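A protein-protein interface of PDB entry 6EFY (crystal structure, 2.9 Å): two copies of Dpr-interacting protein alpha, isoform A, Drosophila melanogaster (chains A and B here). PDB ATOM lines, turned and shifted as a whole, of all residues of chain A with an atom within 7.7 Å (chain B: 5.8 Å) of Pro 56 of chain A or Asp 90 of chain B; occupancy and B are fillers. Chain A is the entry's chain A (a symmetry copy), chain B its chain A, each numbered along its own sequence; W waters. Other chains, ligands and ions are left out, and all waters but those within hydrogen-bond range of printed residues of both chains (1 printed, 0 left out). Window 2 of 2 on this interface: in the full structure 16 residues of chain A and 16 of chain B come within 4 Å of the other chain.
A ring nitrogen (ND1) of His 54 of chain A is in hydrogen-bond range of the backbone carbonyl oxygen (O) of Asn 88 of chain B, 2.8 Å away. O of Ile 52 of chain A is in hydrogen-bond range of ND2 of Asn 88 of chain B, at 2.8 Å.
The side-chain hydroxyl (OG1) of Thr 53 of chain A lies close to the backbone NH (N) of Asn 55 of chain A (3.2 Å). ND2 of Asn 55 of chain A lies close to NH2 of Arg 57 of chain A, at 3.0 Å. O of Gln 45 of chain A lies within hydrogen-bond range of N of Ile 52 of chain A (2.9 Å). The side-chain amide oxygen of Gln 2 of chain B lies close to the side-chain hydroxyl of Tyr 32 of chain B, at 3.3 Å.
His 54 of chain A touches Tyr 32 of chain B. O of His 54 of chain A touches OD2 of Asp 90 of chain B (3.6 Å). OD2 of Asp 90 of chain B touches CA of Asn 55 of chain A (3.3 Å). CD of Pro 56 of chain A touches OD2 of Asp 90 of chain B (3.99 Å).
Printed residues of chain B within 4 Å of Pro 56 of chain A: Asp 90 (3.99 Å). Printed residues of chain A within 4 Å of Tyr 32 of chain B: His 54. Of the printed residues of chain B, His 54 of chain A touches Tyr 32 (3.3 Å), Asn 88 (2.8 Å) and Asp 90 (3.6 Å). Of the printed residues of chain B, Asn 55 of chain A touches Asp 90. Of the printed residues of chain B, Ile 52 of chain A touches Asn 88. Of the printed residues of chain A, Asn 88 of chain B touches Ile 52 (2.8 Å) and His 54 (2.8 Å). The nearest printed residue of chain B that does not touch Pro 56 of chain A is Thr 89 of chain B (8.7 Å). The nearest printed residue of chain A that does not touch Asp 90 of chain B is Thr 53 of chain A (4.7 Å). The nearest printed residue of chain B that does not touch Ile 52 of chain A is Thr 89 of chain B (5.9 Å).
Of the 7 printed residues of chain B, 3 touch a printed residue of chain A. Among the printed residues, 6 pairs touch across the chains. Among the printed residues, no Asp or Glu carboxylate lies within 4 Å of a Lys or Arg side-chain nitrogen of the other chain.
No position is printed for both chains. Of the 6 pairs that touch across the chains among the printed residues, none has its exchanged pair printed and touching as well.
Water W1 lies within hydrogen-bond range of ND2 of Asn 55 of chain A (3.0 Å) and OD1 of Asp 90 of chain B (3.4 Å).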
ATOM      1  N   GLN A  45      16.558 -22.609  10.007  1.00  0.00           N
ATOM      2  CA  GLN A  45      16.908 -22.322  11.392  1.00  0.00           C
ATOM      3  C   GLN A  45      15.932 -22.974  12.365  1.00  0.00           C
ATOM      4  O   GLN A  45      16.351 -23.690  13.282  1.00  0.00           O
ATOM      5  CB  GLN A  45      16.963 -20.809  11.626  1.00  0.00           C
ATOM      6  CG  GLN A  45      18.000 -20.089  10.778  1.00  0.00           C
ATOM      7  CD  GLN A  45      19.396 -20.659  10.947  1.00  0.00           C
ATOM      8  OE1 GLN A  45      20.039 -20.465  11.979  1.00  0.00           O
ATOM      9  NE2 GLN A  45      19.875 -21.366   9.928  1.00  0.00           N
ATOM     10  N   VAL A  51      13.993 -26.045  17.209  1.00  0.00           N
ATOM     11  CA  VAL A  51      15.210 -25.509  16.609  1.00  0.00           C
ATOM     12  C   VAL A  51      15.855 -26.604  15.775  1.00  0.00           C
ATOM     13  O   VAL A  51      16.060 -27.722  16.260  1.00  0.00           O
ATOM     14  CB  VAL A  51      16.182 -24.989  17.681  1.00  0.00           C
ATOM     15  CG1 VAL A  51      17.473 -24.507  17.035  1.00  0.00           C
ATOM     16  CG2 VAL A  51      15.535 -23.879  18.480  1.00  0.00           C
ATOM     17  N   ILE A  52      16.177 -26.287  14.526  1.00  0.00           N
ATOM     18  CA  ILE A  52      16.700 -27.272  13.586  1.00  0.00           C
ATOM     19  C   ILE A  52      18.209 -27.155  13.437  1.00  0.00           C
ATOM     20  O   ILE A  52      18.924 -28.155  13.511  1.00  0.00           O
ATOM     21  CB  ILE A  52      15.983 -27.148  12.222  1.00  0.00           C
ATOM     22  CG1 ILE A  52      14.577 -27.746  12.295  1.00  0.00           C
ATOM     23  CG2 ILE A  52      16.775 -27.843  11.131  1.00  0.00           C
ATOM     24  CD1 ILE A  52      13.550 -26.852  12.942  1.00  0.00           C
ATOM     25  N   THR A  53      18.715 -25.942  13.238  1.00  0.00           N
ATOM     26  CA  THR A  53      20.150 -25.765  13.065  1.00  0.00           C
ATOM     27  C   THR A  53      20.884 -26.074  14.363  1.00  0.00           C
ATOM     28  O   THR A  53      20.384 -25.804  15.459  1.00  0.00           O
ATOM     29  CB  THR A  53      20.468 -24.342  12.612  1.00  0.00           C
ATOM     30  OG1 THR A  53      21.885 -24.200  12.454  1.00  0.00           O
ATOM     31  CG2 THR A  53      19.969 -23.333  13.628  1.00  0.00           C
ATOM     32  N   HIS A  54      22.071 -26.664  14.237  1.00  0.00           N
ATOM     33  CA  HIS A  54      22.911 -26.940  15.389  1.00  0.00           C
ATOM     34  C   HIS A  54      23.867 -25.796  15.696  1.00  0.00           C
ATOM     35  O   HIS A  54      24.834 -25.988  16.444  1.00  0.00           O
ATOM     36  CB  HIS A  54      23.668 -28.252  15.191  1.00  0.00           C
ATOM     37  CG  HIS A  54      22.834 -29.463  15.471  1.00  0.00           C
ATOM     38  ND1 HIS A  54      21.936 -29.974  14.558  1.00  0.00           N
ATOM     39  CD2 HIS A  54      22.738 -30.245  16.572  1.00  0.00           C
ATOM     40  CE1 HIS A  54      21.334 -31.028  15.080  1.00  0.00           C
ATOM     41  NE2 HIS A  54      21.803 -31.214  16.301  1.00  0.00           N
ATOM     42  N   ASN A  55      23.620 -24.624  15.135  1.00  0.00           N
ATOM     43  CA  ASN A  55      24.274 -23.405  15.577  1.00  0.00           C
ATOM     44  C   ASN A  55      23.761 -23.081  16.973  1.00  0.00           C
ATOM     45  O   ASN A  55      22.571 -22.768  17.122  1.00  0.00           O
ATOM     46  CB  ASN A  55      23.978 -22.263  14.606  1.00  0.00           C
ATOM     47  CG  ASN A  55      24.844 -21.043  14.851  1.00  0.00           C
ATOM     48  OD1 ASN A  55      25.259 -20.773  15.977  1.00  0.00           O
ATOM     49  ND2 ASN A  55      25.118 -20.295  13.789  1.00  0.00           N
ATOM     50  N   PRO A  56      24.596 -23.146  18.014  1.00  0.00           N
ATOM     51  CA  PRO A  56      24.066 -23.003  19.380  1.00  0.00           C
ATOM     52  C   PRO A  56      23.525 -21.618  19.685  1.00  0.00           C
ATOM     53  O   PRO A  56      22.629 -21.493  20.527  1.00  0.00           O
ATOM     54  CB  PRO A  56      25.275 -23.345  20.261  1.00  0.00           C
ATOM     55  CG  PRO A  56      26.462 -23.046  19.404  1.00  0.00           C
ATOM     56  CD  PRO A  56      26.051 -23.384  18.001  1.00  0.00           C
ATOM     57  N   ARG A  57      24.023 -20.578  19.018  1.00  0.00           N
ATOM     58  CA  ARG A  57      23.605 -19.209  19.301  1.00  0.00           C
ATOM     59  C   ARG A  57      22.181 -18.901  18.848  1.00  0.00           C
ATOM     60  O   ARG A  57      21.737 -17.759  19.016  1.00  0.00           O
ATOM     61  CB  ARG A  57      24.573 -18.230  18.636  1.00  0.00           C
ATOM     62  CG  ARG A  57      26.037 -18.581  18.839  1.00  0.00           C
ATOM     63  CD  ARG A  57      26.952 -17.554  18.197  1.00  0.00           C
ATOM     64  NE  ARG A  57      26.747 -17.453  16.756  1.00  0.00           N
ATOM     65  CZ  ARG A  57      27.287 -18.280  15.867  1.00  0.00           C
ATOM     66  NH1 ARG A  57      28.062 -19.279  16.264  1.00  0.00           N
ATOM     67  NH2 ARG A  57      27.049 -18.111  14.575  1.00  0.00           N
ATOM     68  N   VAL A  58      21.455 -19.871  18.296  1.00  0.00           N
ATOM     69  CA  VAL A  58      20.159 -19.642  17.669  1.00  0.00           C
ATOM     70  C   VAL A  58      19.072 -20.232  18.556  1.00  0.00           C
ATOM     71  O   VAL A  58      19.139 -21.411  18.931  1.00  0.00           O
ATOM     72  CB  VAL A  58      20.114 -20.252  16.255  1.00  0.00           C
ATOM     73  CG1 VAL A  58      18.804 -19.907  15.561  1.00  0.00           C
ATOM     74  CG2 VAL A  58      21.312 -19.783  15.433  1.00  0.00           C
ATOM     75  N   THR A  59      18.071 -19.416  18.889  1.00  0.00           N
ATOM     76  CA  THR A  59      16.964 -19.841  19.734  1.00  0.00           C
ATOM     77  C   THR A  59      15.666 -19.241  19.209  1.00  0.00           C
ATOM     78  O   THR A  59      15.668 -18.287  18.428  1.00  0.00           O
ATOM     79  CB  THR A  59      17.159 -19.424  21.202  1.00  0.00           C
ATOM     80  OG1 THR A  59      17.321 -18.001  21.280  1.00  0.00           O
ATOM     81  CG2 THR A  59      18.377 -20.112  21.815  1.00  0.00           C
ATOM     82  N   HIS A  71      16.263 -15.479  17.865  1.00  0.00           N
ATOM     83  CA  HIS A  71      17.314 -14.844  18.651  1.00  0.00           C
ATOM     84  C   HIS A  71      18.677 -15.402  18.269  1.00  0.00           C
ATOM     85  O   HIS A  71      18.863 -16.623  18.221  1.00  0.00           O
ATOM     86  CB  HIS A  71      17.076 -15.040  20.148  1.00  0.00           C
ATOM     87  CG  HIS A  71      15.700 -14.665  20.592  1.00  0.00           C
ATOM     88  ND1 HIS A  71      15.321 -13.359  20.817  1.00  0.00           N
ATOM     89  CD2 HIS A  71      14.609 -15.424  20.855  1.00  0.00           C
ATOM     90  CE1 HIS A  71      14.056 -13.330  21.199  1.00  0.00           C
ATOM     91  NE2 HIS A  71      13.601 -14.570  21.231  1.00  0.00           N
ATOM     92  N   ILE A  72      19.625 -14.506  18.009  1.00  0.00           N
ATOM     93  CA  ILE A  72      21.024 -14.860  17.807  1.00  0.00           C
ATOM     94  C   ILE A  72      21.818 -14.268  18.965  1.00  0.00           C
ATOM     95  O   ILE A  72      21.806 -13.048  19.179  1.00  0.00           O
ATOM     96  CB  ILE A  72      21.558 -14.366  16.454  1.00  0.00           C
ATOM     97  CG1 ILE A  72      20.643 -14.811  15.312  1.00  0.00           C
ATOM     98  CG2 ILE A  72      22.955 -14.900  16.218  1.00  0.00           C
ATOM     99  CD1 ILE A  72      19.682 -13.744  14.833  1.00  0.00           C
ATOM    100  N   LYS A  73      22.504 -15.131  19.709  1.00  0.00           N
ATOM    101  CA  LYS A  73      23.255 -14.740  20.894  1.00  0.00           C
ATOM    102  C   LYS A  73      24.720 -14.545  20.524  1.00  0.00           C
ATOM    103  O   LYS A  73      25.365 -15.477  20.030  1.00  0.00           O
ATOM    104  CB  LYS A  73      23.112 -15.798  21.988  1.00  0.00           C
ATOM    105  CG  LYS A  73      24.063 -15.620  23.151  1.00  0.00           C
ATOM    106  CD  LYS A  73      23.874 -16.727  24.177  1.00  0.00           C
ATOM    107  CE  LYS A  73      24.911 -16.638  25.287  1.00  0.00           C
ATOM    108  NZ  LYS A  73      24.922 -15.295  25.921  1.00  0.00           N
ATOM    109  N   ASP A  79      26.873 -14.813  10.821  1.00  0.00           N
ATOM    110  CA  ASP A  79      25.443 -14.673  11.059  1.00  0.00           C
ATOM    111  C   ASP A  79      24.810 -13.586  10.205  1.00  0.00           C
ATOM    112  O   ASP A  79      23.584 -13.554  10.078  1.00  0.00           O
ATOM    113  CB  ASP A  79      25.177 -14.376  12.537  1.00  0.00           C
ATOM    114  CG  ASP A  79      25.688 -15.469  13.448  1.00  0.00           C
ATOM    115  OD1 ASP A  79      25.923 -16.590  12.951  1.00  0.00           O
ATOM    116  OD2 ASP A  79      25.851 -15.207  14.662  1.00  0.00           O
ATOM    117  N   GLN B   2      30.843 -37.403  11.289  1.00  0.00           N
ATOM    118  CA  GLN B   2      29.828 -36.432  10.920  1.00  0.00           C
ATOM    119  C   GLN B   2      28.962 -36.992   9.794  1.00  0.00           C
ATOM    120  O   GLN B   2      29.455 -37.734   8.939  1.00  0.00           O
ATOM    121  CB  GLN B   2      30.465 -35.112  10.463  1.00  0.00           C
ATOM    122  CG  GLN B   2      29.568 -33.887  10.602  1.00  0.00           C
ATOM    123  CD  GLN B   2      29.492 -33.375  12.029  1.00  0.00           C
ATOM    124  OE1 GLN B   2      28.512 -32.745  12.426  1.00  0.00           O
ATOM    125  NE2 GLN B   2      30.537 -33.637  12.804  1.00  0.00           N
ATOM    126  N   TYR B  32      21.052 -36.206  13.574  1.00  0.00           N
ATOM    127  CA  TYR B  32      20.726 -35.039  12.769  1.00  0.00           C
ATOM    128  C   TYR B  32      19.512 -35.330  11.891  1.00  0.00           C
ATOM    129  O   TYR B  32      19.149 -36.485  11.658  1.00  0.00           O
ATOM    130  CB  TYR B  32      21.924 -34.622  11.913  1.00  0.00           C
ATOM    131  CG  TYR B  32      23.082 -34.048  12.704  1.00  0.00           C
ATOM    132  CD1 TYR B  32      22.955 -33.747  14.056  1.00  0.00           C
ATOM    133  CD2 TYR B  32      24.299 -33.797  12.094  1.00  0.00           C
ATOM    134  CE1 TYR B  32      24.019 -33.216  14.776  1.00  0.00           C
ATOM    135  CE2 TYR B  32      25.363 -33.272  12.799  1.00  0.00           C
ATOM    136  CZ  TYR B  32      25.221 -32.981  14.136  1.00  0.00           C
ATOM    137  OH  TYR B  32      26.292 -32.457  14.822  1.00  0.00           O
ATOM    138  N   ASN B  88      20.903 -30.723   9.066  1.00  0.00           N
ATOM    139  CA  ASN B  88      21.004 -29.587   9.979  1.00  0.00           C
ATOM    140  C   ASN B  88      22.318 -29.561  10.754  1.00  0.00           C
ATOM    141  O   ASN B  88      22.339 -29.202  11.933  1.00  0.00           O
ATOM    142  CB  ASN B  88      19.808 -29.589  10.927  1.00  0.00           C
ATOM    143  CG  ASN B  88      19.729 -30.844  11.767  1.00  0.00           C
ATOM    144  OD1 ASN B  88      20.464 -31.802  11.540  1.00  0.00           O
ATOM    145  ND2 ASN B  88      18.824 -30.849  12.741  1.00  0.00           N
ATOM    146  N   THR B  89      23.425 -29.939  10.108  1.00  0.00           N
ATOM    147  CA  THR B  89      24.751 -29.803  10.700  1.00  0.00           C
ATOM    148  C   THR B  89      25.083 -28.326  10.863  1.00  0.00           C
ATOM    149  O   THR B  89      24.312 -27.455  10.445  1.00  0.00           O
ATOM    150  CB  THR B  89      25.815 -30.485   9.833  1.00  0.00           C
ATOM    151  OG1 THR B  89      26.009 -29.733   8.629  1.00  0.00           O
ATOM    152  CG2 THR B  89      25.387 -31.890   9.457  1.00  0.00           C
ATOM    153  N   ASP B  90      26.227 -28.028  11.468  1.00  0.00           N
ATOM    154  CA  ASP B  90      26.659 -26.642  11.597  1.00  0.00           C
ATOM    155  C   ASP B  90      28.120 -26.518  11.172  1.00  0.00           C
ATOM    156  O   ASP B  90      29.015 -26.931  11.906  1.00  0.00           O
ATOM    157  CB  ASP B  90      26.464 -26.144  13.030  1.00  0.00           C
ATOM    158  CG  ASP B  90      26.749 -24.658  13.175  1.00  0.00           C
ATOM    159  OD1 ASP B  90      26.547 -23.906  12.192  1.00  0.00           O
ATOM    160  OD2 ASP B  90      27.174 -24.240  14.274  1.00  0.00           O
ATOM    161  N   PRO B  91      28.366 -25.951   9.976  1.00  0.00           N
ATOM    162  CA  PRO B  91      27.351 -25.442   9.047  1.00  0.00           C
ATOM    163  C   PRO B  91      26.631 -26.563   8.302  1.00  0.00           C
ATOM    164  O   PRO B  91      27.120 -27.693   8.281  1.00  0.00           O
ATOM    165  CB  PRO B  91      28.167 -24.578   8.086  1.00  0.00           C
ATOM    166  CG  PRO B  91      29.498 -25.236   8.055  1.00  0.00           C
ATOM    167  CD  PRO B  91      29.729 -25.784   9.440  1.00  0.00           C
ATOM    168  N   MET B  92      25.482 -26.252   7.707  1.00  0.00           N
ATOM    169  CA  MET B  92      24.663 -27.275   7.076  1.00  0.00           C
ATOM    170  C   MET B  92      25.231 -27.667   5.720  1.00  0.00           C
ATOM    171  O   MET B  92      25.861 -26.864   5.025  1.00  0.00           O
ATOM    172  CB  MET B  92      23.217 -26.795   6.922  1.00  0.00           C
ATOM    173  CG  MET B  92      22.979 -25.795   5.802  1.00  0.00           C
ATOM    174  SD  MET B  92      22.519 -26.557   4.234  1.00  0.00           S
ATOM    175  CE  MET B  92      21.204 -25.474   3.694  1.00  0.00           C
HETATM  176  O   HOH W   1      26.837 -20.627  11.351  1.00  0.00           O
